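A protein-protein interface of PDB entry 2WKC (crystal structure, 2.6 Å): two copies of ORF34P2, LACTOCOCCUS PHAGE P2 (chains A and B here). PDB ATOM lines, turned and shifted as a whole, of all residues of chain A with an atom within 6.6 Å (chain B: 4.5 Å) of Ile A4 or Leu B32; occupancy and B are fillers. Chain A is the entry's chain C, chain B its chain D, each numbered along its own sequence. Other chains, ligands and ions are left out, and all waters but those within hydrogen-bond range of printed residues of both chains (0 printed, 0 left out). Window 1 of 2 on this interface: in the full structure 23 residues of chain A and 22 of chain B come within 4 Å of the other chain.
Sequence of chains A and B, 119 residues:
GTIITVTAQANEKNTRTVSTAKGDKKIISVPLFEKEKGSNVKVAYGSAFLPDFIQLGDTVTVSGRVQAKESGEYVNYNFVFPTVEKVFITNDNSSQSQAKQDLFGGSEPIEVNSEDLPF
The side-chain hydroxyl of Thr A2 lies within hydrogen-bond range of the backbone carbonyl oxygen of Pro B31 (2.7 Å).
The backbone NH (N) of Thr A5 is in hydrogen-bond range of the backbone carbonyl oxygen (O) of Ile B3 (2.9 Å).
The backbone carbonyl oxygen of Pro A31 sits at hydrogen-bond distance from the side-chain hydroxyl of Thr B2, at 3.2 Å.
The backbone NH (N) of Gly A64 lies within hydrogen-bond range of the backbone carbonyl oxygen (O) of Ile A4.
The side-chain hydroxyl (OG1) of Thr A5 is in hydrogen-bond range of the side-chain hydroxyl (OG) of Ser A63 (3.1 Å).
O of Val A62 lies within hydrogen-bond range of N of Val A6.
The backbone NH (N) of Leu B32 sits at hydrogen-bond distance from the backbone carbonyl oxygen (O) of Ala B44 (3.1 Å).
Thr A2 touches Ile B4 (CG2 to CG2, 3.8 Å).
Thr A2 touches Leu B32 (CG2 to O, 3.2 Å).
Ile B3 touches Ile A3 (O to O, 3.9 Å).
Ile A3 touches Ile B4 (O to CA, 3.5 Å).
Ile B3 touches Ile A4 (O to CA, 3.7 Å).
Thr A5 touches Thr B2.
Val A6 touches Thr B2 (CG1 to OG1, 3.7 Å).
Thr B2 touches Leu A32.
CD1 of Ile B4 touches O of Leu A32 (3.4 Å).
Val B66 touches Phe A33 (O to CB, 3.5 Å).
Printed residues of chain B within 4 Å of Ile A4: Ile B3 (3.7 Å) and Leu B32 (3.2 Å).
Printed residues of chain B within 4 Å of Leu A32: Thr B2 and Ile B4.
Arg A65 touches none of the printed residues of chain B.
Printed residues of chain B within 4 Å of Val A66: Phe B33 (3.6 Å).
Printed residues of chain A within 4 Å of Pro B31: Thr A2 (2.7 Å).
Of the printed residues of chain A, Leu B32 touches Thr A2 (3.2 Å) and Ile A4 (3.2 Å).
Of the printed residues of chain A, Val B66 touches Phe A33.
The nearest residue of chain A that does not touch Leu B32 is Phe A33 (4.8 Å).
The nearest printed residue of chain A that does not touch Ile B3 is Val A6 (5.2 Å).
Of the 14 printed residues of chain A, 9 touch a printed residue of chain B.
Printed residues of chain A that touch a printed residue of chain B: Thr A2, Ile A3, Ile A4, Thr A5, Val A6, Pro A31, Leu A32, Phe A33 and Val A66.
Hydrophobic or aromatic side chains of chain A within 4 Å of the printed part of chain B: Ile A4, Val A6 and Phe A33.
Along chain A the printed residues that touch a printed residue of chain B span positions 2 to 66.
Among the printed residues, no Asp or Glu carboxylate lies within 4 Å of a Lys or Arg side-chain nitrogen of the other chain.
Thr A2 touches Leu B32, and with the chains exchanged Leu A32 touches Thr B2.
Ile B3 touches its own counterpart, Ile A3.
Ile A4 touches Leu B32, and with the chains exchanged Leu A32 touches Ile B4.
Phe A33 touches Val B66, and with the chains exchanged Val A66 touches Phe B33.
Of the 16 pairs that touch across the chains among the printed residues, 11 have their exchanged pair printed and touching as well.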
ATOM      1  N   THR A   2      -4.377  19.706   2.053  1.00  0.00           N
ATOM      2  CA  THR A   2      -4.137  18.817   0.920  1.00  0.00           C
ATOM      3  C   THR A   2      -5.360  18.700   0.022  1.00  0.00           C
ATOM      4  O   THR A   2      -6.449  18.379   0.495  1.00  0.00           O
ATOM      5  CB  THR A   2      -3.749  17.398   1.403  1.00  0.00           C
ATOM      6  OG1 THR A   2      -2.646  17.483   2.311  1.00  0.00           O
ATOM      7  CG2 THR A   2      -3.372  16.503   0.235  1.00  0.00           C
ATOM      8  N   ILE A   3      -5.164  18.954  -1.272  1.00  0.00           N
ATOM      9  CA  ILE A   3      -6.197  18.753  -2.294  1.00  0.00           C
ATOM     10  C   ILE A   3      -5.777  17.614  -3.223  1.00  0.00           C
ATOM     11  O   ILE A   3      -4.659  17.580  -3.718  1.00  0.00           O
ATOM     12  CB  ILE A   3      -6.468  20.055  -3.120  1.00  0.00           C
ATOM     13  CG1 ILE A   3      -7.092  21.146  -2.241  1.00  0.00           C
ATOM     14  CG2 ILE A   3      -7.357  19.779  -4.347  1.00  0.00           C
ATOM     15  CD1 ILE A   3      -8.519  20.884  -1.800  1.00  0.00           C
ATOM     16  N   ILE A   4      -6.685  16.680  -3.451  1.00  0.00           N
ATOM     17  CA  ILE A   4      -6.423  15.550  -4.324  1.00  0.00           C
ATOM     18  C   ILE A   4      -7.398  15.590  -5.490  1.00  0.00           C
ATOM     19  O   ILE A   4      -8.618  15.661  -5.279  1.00  0.00           O
ATOM     20  CB  ILE A   4      -6.543  14.219  -3.559  1.00  0.00           C
ATOM     21  CG1 ILE A   4      -5.491  14.168  -2.443  1.00  0.00           C
ATOM     22  CG2 ILE A   4      -6.418  13.034  -4.524  1.00  0.00           C
ATOM     23  CD1 ILE A   4      -5.518  12.917  -1.573  1.00  0.00           C
ATOM     24  N   THR A   5      -6.846  15.545  -6.705  1.00  0.00           N
ATOM     25  CA  THR A   5      -7.603  15.608  -7.958  1.00  0.00           C
ATOM     26  C   THR A   5      -7.360  14.327  -8.766  1.00  0.00           C
ATOM     27  O   THR A   5      -6.242  14.087  -9.230  1.00  0.00           O
ATOM     28  CB  THR A   5      -7.189  16.861  -8.796  1.00  0.00           C
ATOM     29  OG1 THR A   5      -7.504  18.053  -8.070  1.00  0.00           O
ATOM     30  CG2 THR A   5      -7.903  16.909 -10.140  1.00  0.00           C
ATOM     31  N   VAL A   6      -8.402  13.515  -8.932  1.00  0.00           N
ATOM     32  CA  VAL A   6      -8.287  12.216  -9.614  1.00  0.00           C
ATOM     33  C   VAL A   6      -9.154  12.188 -10.870  1.00  0.00           C
ATOM     34  O   VAL A   6     -10.262  12.708 -10.870  1.00  0.00           O
ATOM     35  CB  VAL A   6      -8.742  11.020  -8.709  1.00  0.00           C
ATOM     36  CG1 VAL A   6      -8.114   9.700  -9.177  1.00  0.00           C
ATOM     37  CG2 VAL A   6      -8.419  11.271  -7.251  1.00  0.00           C
ATOM     38  N   PRO A  31      -8.316   6.052  -6.795  1.00  0.00           N
ATOM     39  CA  PRO A  31      -6.982   5.933  -6.172  1.00  0.00           C
ATOM     40  C   PRO A  31      -6.384   7.253  -5.673  1.00  0.00           C
ATOM     41  O   PRO A  31      -6.482   8.270  -6.351  1.00  0.00           O
ATOM     42  CB  PRO A  31      -6.120   5.354  -7.298  1.00  0.00           C
ATOM     43  CG  PRO A  31      -6.835   5.733  -8.558  1.00  0.00           C
ATOM     44  CD  PRO A  31      -8.284   5.722  -8.235  1.00  0.00           C
ATOM     45  N   LEU A  32      -5.749   7.221  -4.502  1.00  0.00           N
ATOM     46  CA  LEU A  32      -5.202   8.439  -3.895  1.00  0.00           C
ATOM     47  C   LEU A  32      -3.753   8.737  -4.262  1.00  0.00           C
ATOM     48  O   LEU A  32      -3.247   9.812  -3.970  1.00  0.00           O
ATOM     49  CB  LEU A  32      -5.399   8.448  -2.372  1.00  0.00           C
ATOM     50  CG  LEU A  32      -6.839   8.198  -1.891  1.00  0.00           C
ATOM     51  CD1 LEU A  32      -6.948   8.321  -0.381  1.00  0.00           C
ATOM     52  CD2 LEU A  32      -7.855   9.094  -2.597  1.00  0.00           C
ATOM     53  N   PHE A  33      -3.084   7.784  -4.900  1.00  0.00           N
ATOM     54  CA  PHE A  33      -1.762   8.035  -5.471  1.00  0.00           C
ATOM     55  C   PHE A  33      -1.436   6.957  -6.478  1.00  0.00           C
ATOM     56  O   PHE A  33      -2.229   6.054  -6.691  1.00  0.00           O
ATOM     57  CB  PHE A  33      -0.658   8.172  -4.404  1.00  0.00           C
ATOM     58  CG  PHE A  33      -0.848   7.294  -3.199  1.00  0.00           C
ATOM     59  CD1 PHE A  33      -0.416   5.977  -3.207  1.00  0.00           C
ATOM     60  CD2 PHE A  33      -1.438   7.801  -2.044  1.00  0.00           C
ATOM     61  CE1 PHE A  33      -0.589   5.160  -2.084  1.00  0.00           C
ATOM     62  CE2 PHE A  33      -1.615   7.003  -0.924  1.00  0.00           C
ATOM     63  CZ  PHE A  33      -1.188   5.675  -0.944  1.00  0.00           C
ATOM     64  N   VAL A  62     -12.668  13.838  -9.918  1.00  0.00           N
ATOM     65  CA  VAL A  62     -13.070  13.983  -8.525  1.00  0.00           C
ATOM     66  C   VAL A  62     -11.965  14.776  -7.828  1.00  0.00           C
ATOM     67  O   VAL A  62     -10.798  14.380  -7.865  1.00  0.00           O
ATOM     68  CB  VAL A  62     -13.245  12.605  -7.822  1.00  0.00           C
ATOM     69  CG1 VAL A  62     -13.702  12.789  -6.394  1.00  0.00           C
ATOM     70  CG2 VAL A  62     -14.219  11.727  -8.564  1.00  0.00           C
ATOM     71  N   SER A  63     -12.335  15.884  -7.191  1.00  0.00           N
ATOM     72  CA  SER A  63     -11.363  16.791  -6.594  1.00  0.00           C
ATOM     73  C   SER A  63     -11.819  17.345  -5.256  1.00  0.00           C
ATOM     74  O   SER A  63     -12.920  17.880  -5.141  1.00  0.00           O
ATOM     75  CB  SER A  63     -11.085  17.951  -7.551  1.00  0.00           C
ATOM     76  OG  SER A  63     -10.264  18.930  -6.944  1.00  0.00           O
ATOM     77  N   GLY A  64     -10.958  17.234  -4.252  1.00  0.00           N
ATOM     78  CA  GLY A  64     -11.209  17.840  -2.945  1.00  0.00           C
ATOM     79  C   GLY A  64     -10.341  17.281  -1.843  1.00  0.00           C
ATOM     80  O   GLY A  64      -9.405  16.528  -2.100  1.00  0.00           O
ATOM     81  N   ARG A  65     -10.655  17.671  -0.612  1.00  0.00           N
ATOM     82  CA  ARG A  65     -10.024  17.146   0.595  1.00  0.00           C
ATOM     83  C   ARG A  65     -10.379  15.701   0.791  1.00  0.00           C
ATOM     84  O   ARG A  65     -11.483  15.296   0.458  1.00  0.00           O
ATOM     85  CB  ARG A  65     -10.568  17.872   1.812  1.00  0.00           C
ATOM     86  CG  ARG A  65     -10.079  19.268   2.001  1.00  0.00           C
ATOM     87  CD  ARG A  65     -10.816  19.914   3.157  1.00  0.00           C
ATOM     88  NE  ARG A  65     -11.042  18.965   4.242  1.00  0.00           N
ATOM     89  CZ  ARG A  65     -11.201  19.309   5.514  1.00  0.00           C
ATOM     90  NH1 ARG A  65     -11.144  20.587   5.870  1.00  0.00           N
ATOM     91  NH2 ARG A  65     -11.401  18.370   6.430  1.00  0.00           N
ATOM     92  N   VAL A  66      -9.462  14.940   1.386  1.00  0.00           N
ATOM     93  CA  VAL A  66      -9.709  13.548   1.761  1.00  0.00           C
ATOM     94  C   VAL A  66      -9.443  13.337   3.249  1.00  0.00           C
ATOM     95  O   VAL A  66      -8.454  13.819   3.802  1.00  0.00           O
ATOM     96  CB  VAL A  66      -8.851  12.599   0.925  1.00  0.00           C
ATOM     97  CG1 VAL A  66      -8.825  11.186   1.522  1.00  0.00           C
ATOM     98  CG2 VAL A  66      -9.353  12.570  -0.505  1.00  0.00           C
ATOM     99  N   PHE A  79     -13.694  11.564   0.431  1.00  0.00           N
ATOM    100  CA  PHE A  79     -13.657  12.941  -0.036  1.00  0.00           C
ATOM    101  C   PHE A  79     -14.716  13.738   0.700  1.00  0.00           C
ATOM    102  O   PHE A  79     -15.821  13.252   0.914  1.00  0.00           O
ATOM    103  CB  PHE A  79     -13.909  13.016  -1.535  1.00  0.00           C
ATOM    104  CG  PHE A  79     -12.739  12.595  -2.366  1.00  0.00           C
ATOM    105  CD1 PHE A  79     -11.897  13.547  -2.930  1.00  0.00           C
ATOM    106  CD2 PHE A  79     -12.478  11.244  -2.593  1.00  0.00           C
ATOM    107  CE1 PHE A  79     -10.802  13.160  -3.713  1.00  0.00           C
ATOM    108  CE2 PHE A  79     -11.391  10.848  -3.357  1.00  0.00           C
ATOM    109  CZ  PHE A  79     -10.552  11.810  -3.923  1.00  0.00           C
ATOM    110  N   THR B   2      -3.577  10.909 -10.836  1.00  0.00           N
ATOM    111  CA  THR B   2      -3.747  11.527  -9.529  1.00  0.00           C
ATOM    112  C   THR B   2      -2.745  12.662  -9.336  1.00  0.00           C
ATOM    113  O   THR B   2      -1.528  12.435  -9.342  1.00  0.00           O
ATOM    114  CB  THR B   2      -3.579  10.475  -8.393  1.00  0.00           C
ATOM    115  OG1 THR B   2      -4.495   9.385  -8.596  1.00  0.00           O
ATOM    116  CG2 THR B   2      -3.811  11.096  -7.031  1.00  0.00           C
ATOM    117  N   ILE B   3      -3.270  13.880  -9.190  1.00  0.00           N
ATOM    118  CA  ILE B   3      -2.481  15.075  -8.862  1.00  0.00           C
ATOM    119  C   ILE B   3      -2.769  15.467  -7.410  1.00  0.00           C
ATOM    120  O   ILE B   3      -3.929  15.577  -7.011  1.00  0.00           O
ATOM    121  CB  ILE B   3      -2.831  16.288  -9.790  1.00  0.00           C
ATOM    122  CG1 ILE B   3      -2.648  15.943 -11.286  1.00  0.00           C
ATOM    123  CG2 ILE B   3      -2.079  17.580  -9.357  1.00  0.00           C
ATOM    124  CD1 ILE B   3      -1.216  15.843 -11.791  1.00  0.00           C
ATOM    125  N   ILE B   4      -1.715  15.671  -6.627  1.00  0.00           N
ATOM    126  CA  ILE B   4      -1.859  16.120  -5.254  1.00  0.00           C
ATOM    127  C   ILE B   4      -1.233  17.499  -5.101  1.00  0.00           C
ATOM    128  O   ILE B   4      -0.081  17.709  -5.490  1.00  0.00           O
ATOM    129  CB  ILE B   4      -1.250  15.102  -4.250  1.00  0.00           C
ATOM    130  CG1 ILE B   4      -1.999  13.766  -4.362  1.00  0.00           C
ATOM    131  CG2 ILE B   4      -1.324  15.643  -2.807  1.00  0.00           C
ATOM    132  CD1 ILE B   4      -1.338  12.595  -3.682  1.00  0.00           C
ATOM    133  N   VAL B  30       5.363  16.294   3.481  1.00  0.00           N
ATOM    134  CA  VAL B  30       4.012  16.887   3.489  1.00  0.00           C
ATOM    135  C   VAL B  30       2.899  15.821   3.582  1.00  0.00           C
ATOM    136  O   VAL B  30       3.015  14.758   2.977  1.00  0.00           O
ATOM    137  CB  VAL B  30       3.751  17.776   2.236  1.00  0.00           C
ATOM    138  CG1 VAL B  30       4.575  19.067   2.277  1.00  0.00           C
ATOM    139  CG2 VAL B  30       4.001  17.005   0.933  1.00  0.00           C
ATOM    140  N   PRO B  31       1.822  16.096   4.352  1.00  0.00           N
ATOM    141  CA  PRO B  31       0.714  15.135   4.498  1.00  0.00           C
ATOM    142  C   PRO B  31      -0.141  14.981   3.239  1.00  0.00           C
ATOM    143  O   PRO B  31      -0.416  15.962   2.550  1.00  0.00           O
ATOM    144  CB  PRO B  31      -0.129  15.739   5.624  1.00  0.00           C
ATOM    145  CG  PRO B  31       0.231  17.174   5.655  1.00  0.00           C
ATOM    146  CD  PRO B  31       1.661  17.257   5.250  1.00  0.00           C
ATOM    147  N   LEU B  32      -0.579  13.758   2.962  1.00  0.00           N
ATOM    148  CA  LEU B  32      -1.302  13.484   1.725  1.00  0.00           C
ATOM    149  C   LEU B  32      -2.807  13.395   1.923  1.00  0.00           C
ATOM    150  O   LEU B  32      -3.555  13.345   0.955  1.00  0.00           O
ATOM    151  CB  LEU B  32      -0.759  12.224   1.046  1.00  0.00           C
ATOM    152  CG  LEU B  32       0.748  12.244   0.784  1.00  0.00           C
ATOM    153  CD1 LEU B  32       1.247  10.857   0.439  1.00  0.00           C
ATOM    154  CD2 LEU B  32       1.117  13.261  -0.295  1.00  0.00           C
ATOM    155  N   PHE B  33      -3.235  13.382   3.181  1.00  0.00           N
ATOM    156  CA  PHE B  33      -4.639  13.446   3.549  1.00  0.00           C
ATOM    157  C   PHE B  33      -4.752  13.817   5.017  1.00  0.00           C
ATOM    158  O   PHE B  33      -3.736  14.015   5.683  1.00  0.00           O
ATOM    159  CB  PHE B  33      -5.346  12.117   3.272  1.00  0.00           C
ATOM    160  CG  PHE B  33      -4.614  10.910   3.791  1.00  0.00           C
ATOM    161  CD1 PHE B  33      -4.785  10.486   5.109  1.00  0.00           C
ATOM    162  CD2 PHE B  33      -3.777  10.176   2.951  1.00  0.00           C
ATOM    163  CE1 PHE B  33      -4.117   9.355   5.590  1.00  0.00           C
ATOM    164  CE2 PHE B  33      -3.111   9.048   3.417  1.00  0.00           C
ATOM    165  CZ  PHE B  33      -3.279   8.632   4.739  1.00  0.00           C
ATOM    166  N   ALA B  44      -0.148   9.164   5.620  1.00  0.00           N
ATOM    167  CA  ALA B  44       0.940   8.955   4.669  1.00  0.00           C
ATOM    168  C   ALA B  44       1.574  10.289   4.300  1.00  0.00           C
ATOM    169  O   ALA B  44       0.872  11.272   4.054  1.00  0.00           O
ATOM    170  CB  ALA B  44       0.447   8.244   3.435  1.00  0.00           C
ATOM    171  N   TYR B  45       2.905  10.314   4.265  1.00  0.00           N
ATOM    172  CA  TYR B  45       3.655  11.528   3.948  1.00  0.00           C
ATOM    173  C   TYR B  45       4.460  11.427   2.647  1.00  0.00           C
ATOM    174  O   TYR B  45       5.157  10.440   2.429  1.00  0.00           O
ATOM    175  CB  TYR B  45       4.569  11.897   5.116  1.00  0.00           C
ATOM    176  CG  TYR B  45       3.803  12.344   6.335  1.00  0.00           C
ATOM    177  CD1 TYR B  45       3.435  13.682   6.501  1.00  0.00           C
ATOM    178  CD2 TYR B  45       3.437  11.430   7.322  1.00  0.00           C
ATOM    179  CE1 TYR B  45       2.715  14.090   7.619  1.00  0.00           C
ATOM    180  CE2 TYR B  45       2.724  11.830   8.440  1.00  0.00           C
ATOM    181  CZ  TYR B  45       2.363  13.158   8.583  1.00  0.00           C
ATOM    182  OH  TYR B  45       1.656  13.547   9.700  1.00  0.00           O
ATOM    183  N   GLY B  46       4.360  12.452   1.796  1.00  0.00           N
ATOM    184  CA  GLY B  46       5.109  12.504   0.537  1.00  0.00           C
ATOM    185  C   GLY B  46       6.324  13.414   0.605  1.00  0.00           C
ATOM    186  O   GLY B  46       6.336  14.394   1.348  1.00  0.00           O
ATOM    187  N   VAL B  66       2.064  11.906  -7.230  1.00  0.00           N
ATOM    188  CA  VAL B  66       2.761  11.190  -6.177  1.00  0.00           C
ATOM    189  C   VAL B  66       2.806   9.717  -6.539  1.00  0.00           C
ATOM    190  O   VAL B  66       1.767   9.092  -6.794  1.00  0.00           O
ATOM    191  CB  VAL B  66       2.110  11.396  -4.814  1.00  0.00           C
ATOM    192  CG1 VAL B  66       2.782  10.515  -3.760  1.00  0.00           C
ATOM    193  CG2 VAL B  66       2.188  12.867  -4.413  1.00  0.00           C
ATOM    194  N   TYR B  77       6.608   7.471  -0.578  1.00  0.00           N
ATOM    195  CA  TYR B  77       5.738   8.319  -1.372  1.00  0.00           C
ATOM    196  C   TYR B  77       6.508   9.547  -1.827  1.00  0.00           C
ATOM    197  O   TYR B  77       6.836  10.423  -1.023  1.00  0.00           O
ATOM    198  CB  TYR B  77       4.512   8.725  -0.568  1.00  0.00           C
ATOM    199  CG  TYR B  77       3.783   7.568   0.068  1.00  0.00           C
ATOM    200  CD1 TYR B  77       2.864   6.811  -0.664  1.00  0.00           C
ATOM    201  CD2 TYR B  77       4.009   7.233   1.408  1.00  0.00           C
ATOM    202  CE1 TYR B  77       2.187   5.754  -0.076  1.00  0.00           C
ATOM    203  CE2 TYR B  77       3.342   6.178   2.001  1.00  0.00           C
ATOM    204  CZ  TYR B  77       2.428   5.442   1.257  1.00  0.00           C
ATOM    205  OH  TYR B  77       1.769   4.386   1.844  1.00  0.00           O
ATOM    206  N   PHE B  79       7.090  12.751  -4.685  1.00  0.00           N
ATOM    207  CA  PHE B  79       6.575  13.632  -5.720  1.00  0.00           C
ATOM    208  C   PHE B  79       7.492  13.508  -6.928  1.00  0.00           C
ATOM    209  O   PHE B  79       8.711  13.547  -6.796  1.00  0.00           O
ATOM    210  CB  PHE B  79       6.509  15.082  -5.228  1.00  0.00           C
ATOM    211  CG  PHE B  79       5.288  15.398  -4.397  1.00  0.00           C
ATOM    212  CD1 PHE B  79       4.183  16.022  -4.969  1.00  0.00           C
ATOM    213  CD2 PHE B  79       5.251  15.098  -3.036  1.00  0.00           C
ATOM    214  CE1 PHE B  79       3.050  16.333  -4.200  1.00  0.00           C
ATOM    215  CE2 PHE B  79       4.123  15.406  -2.258  1.00  0.00           C
ATOM    216  CZ  PHE B  79       3.021  16.022  -2.839  1.00  0.00           C
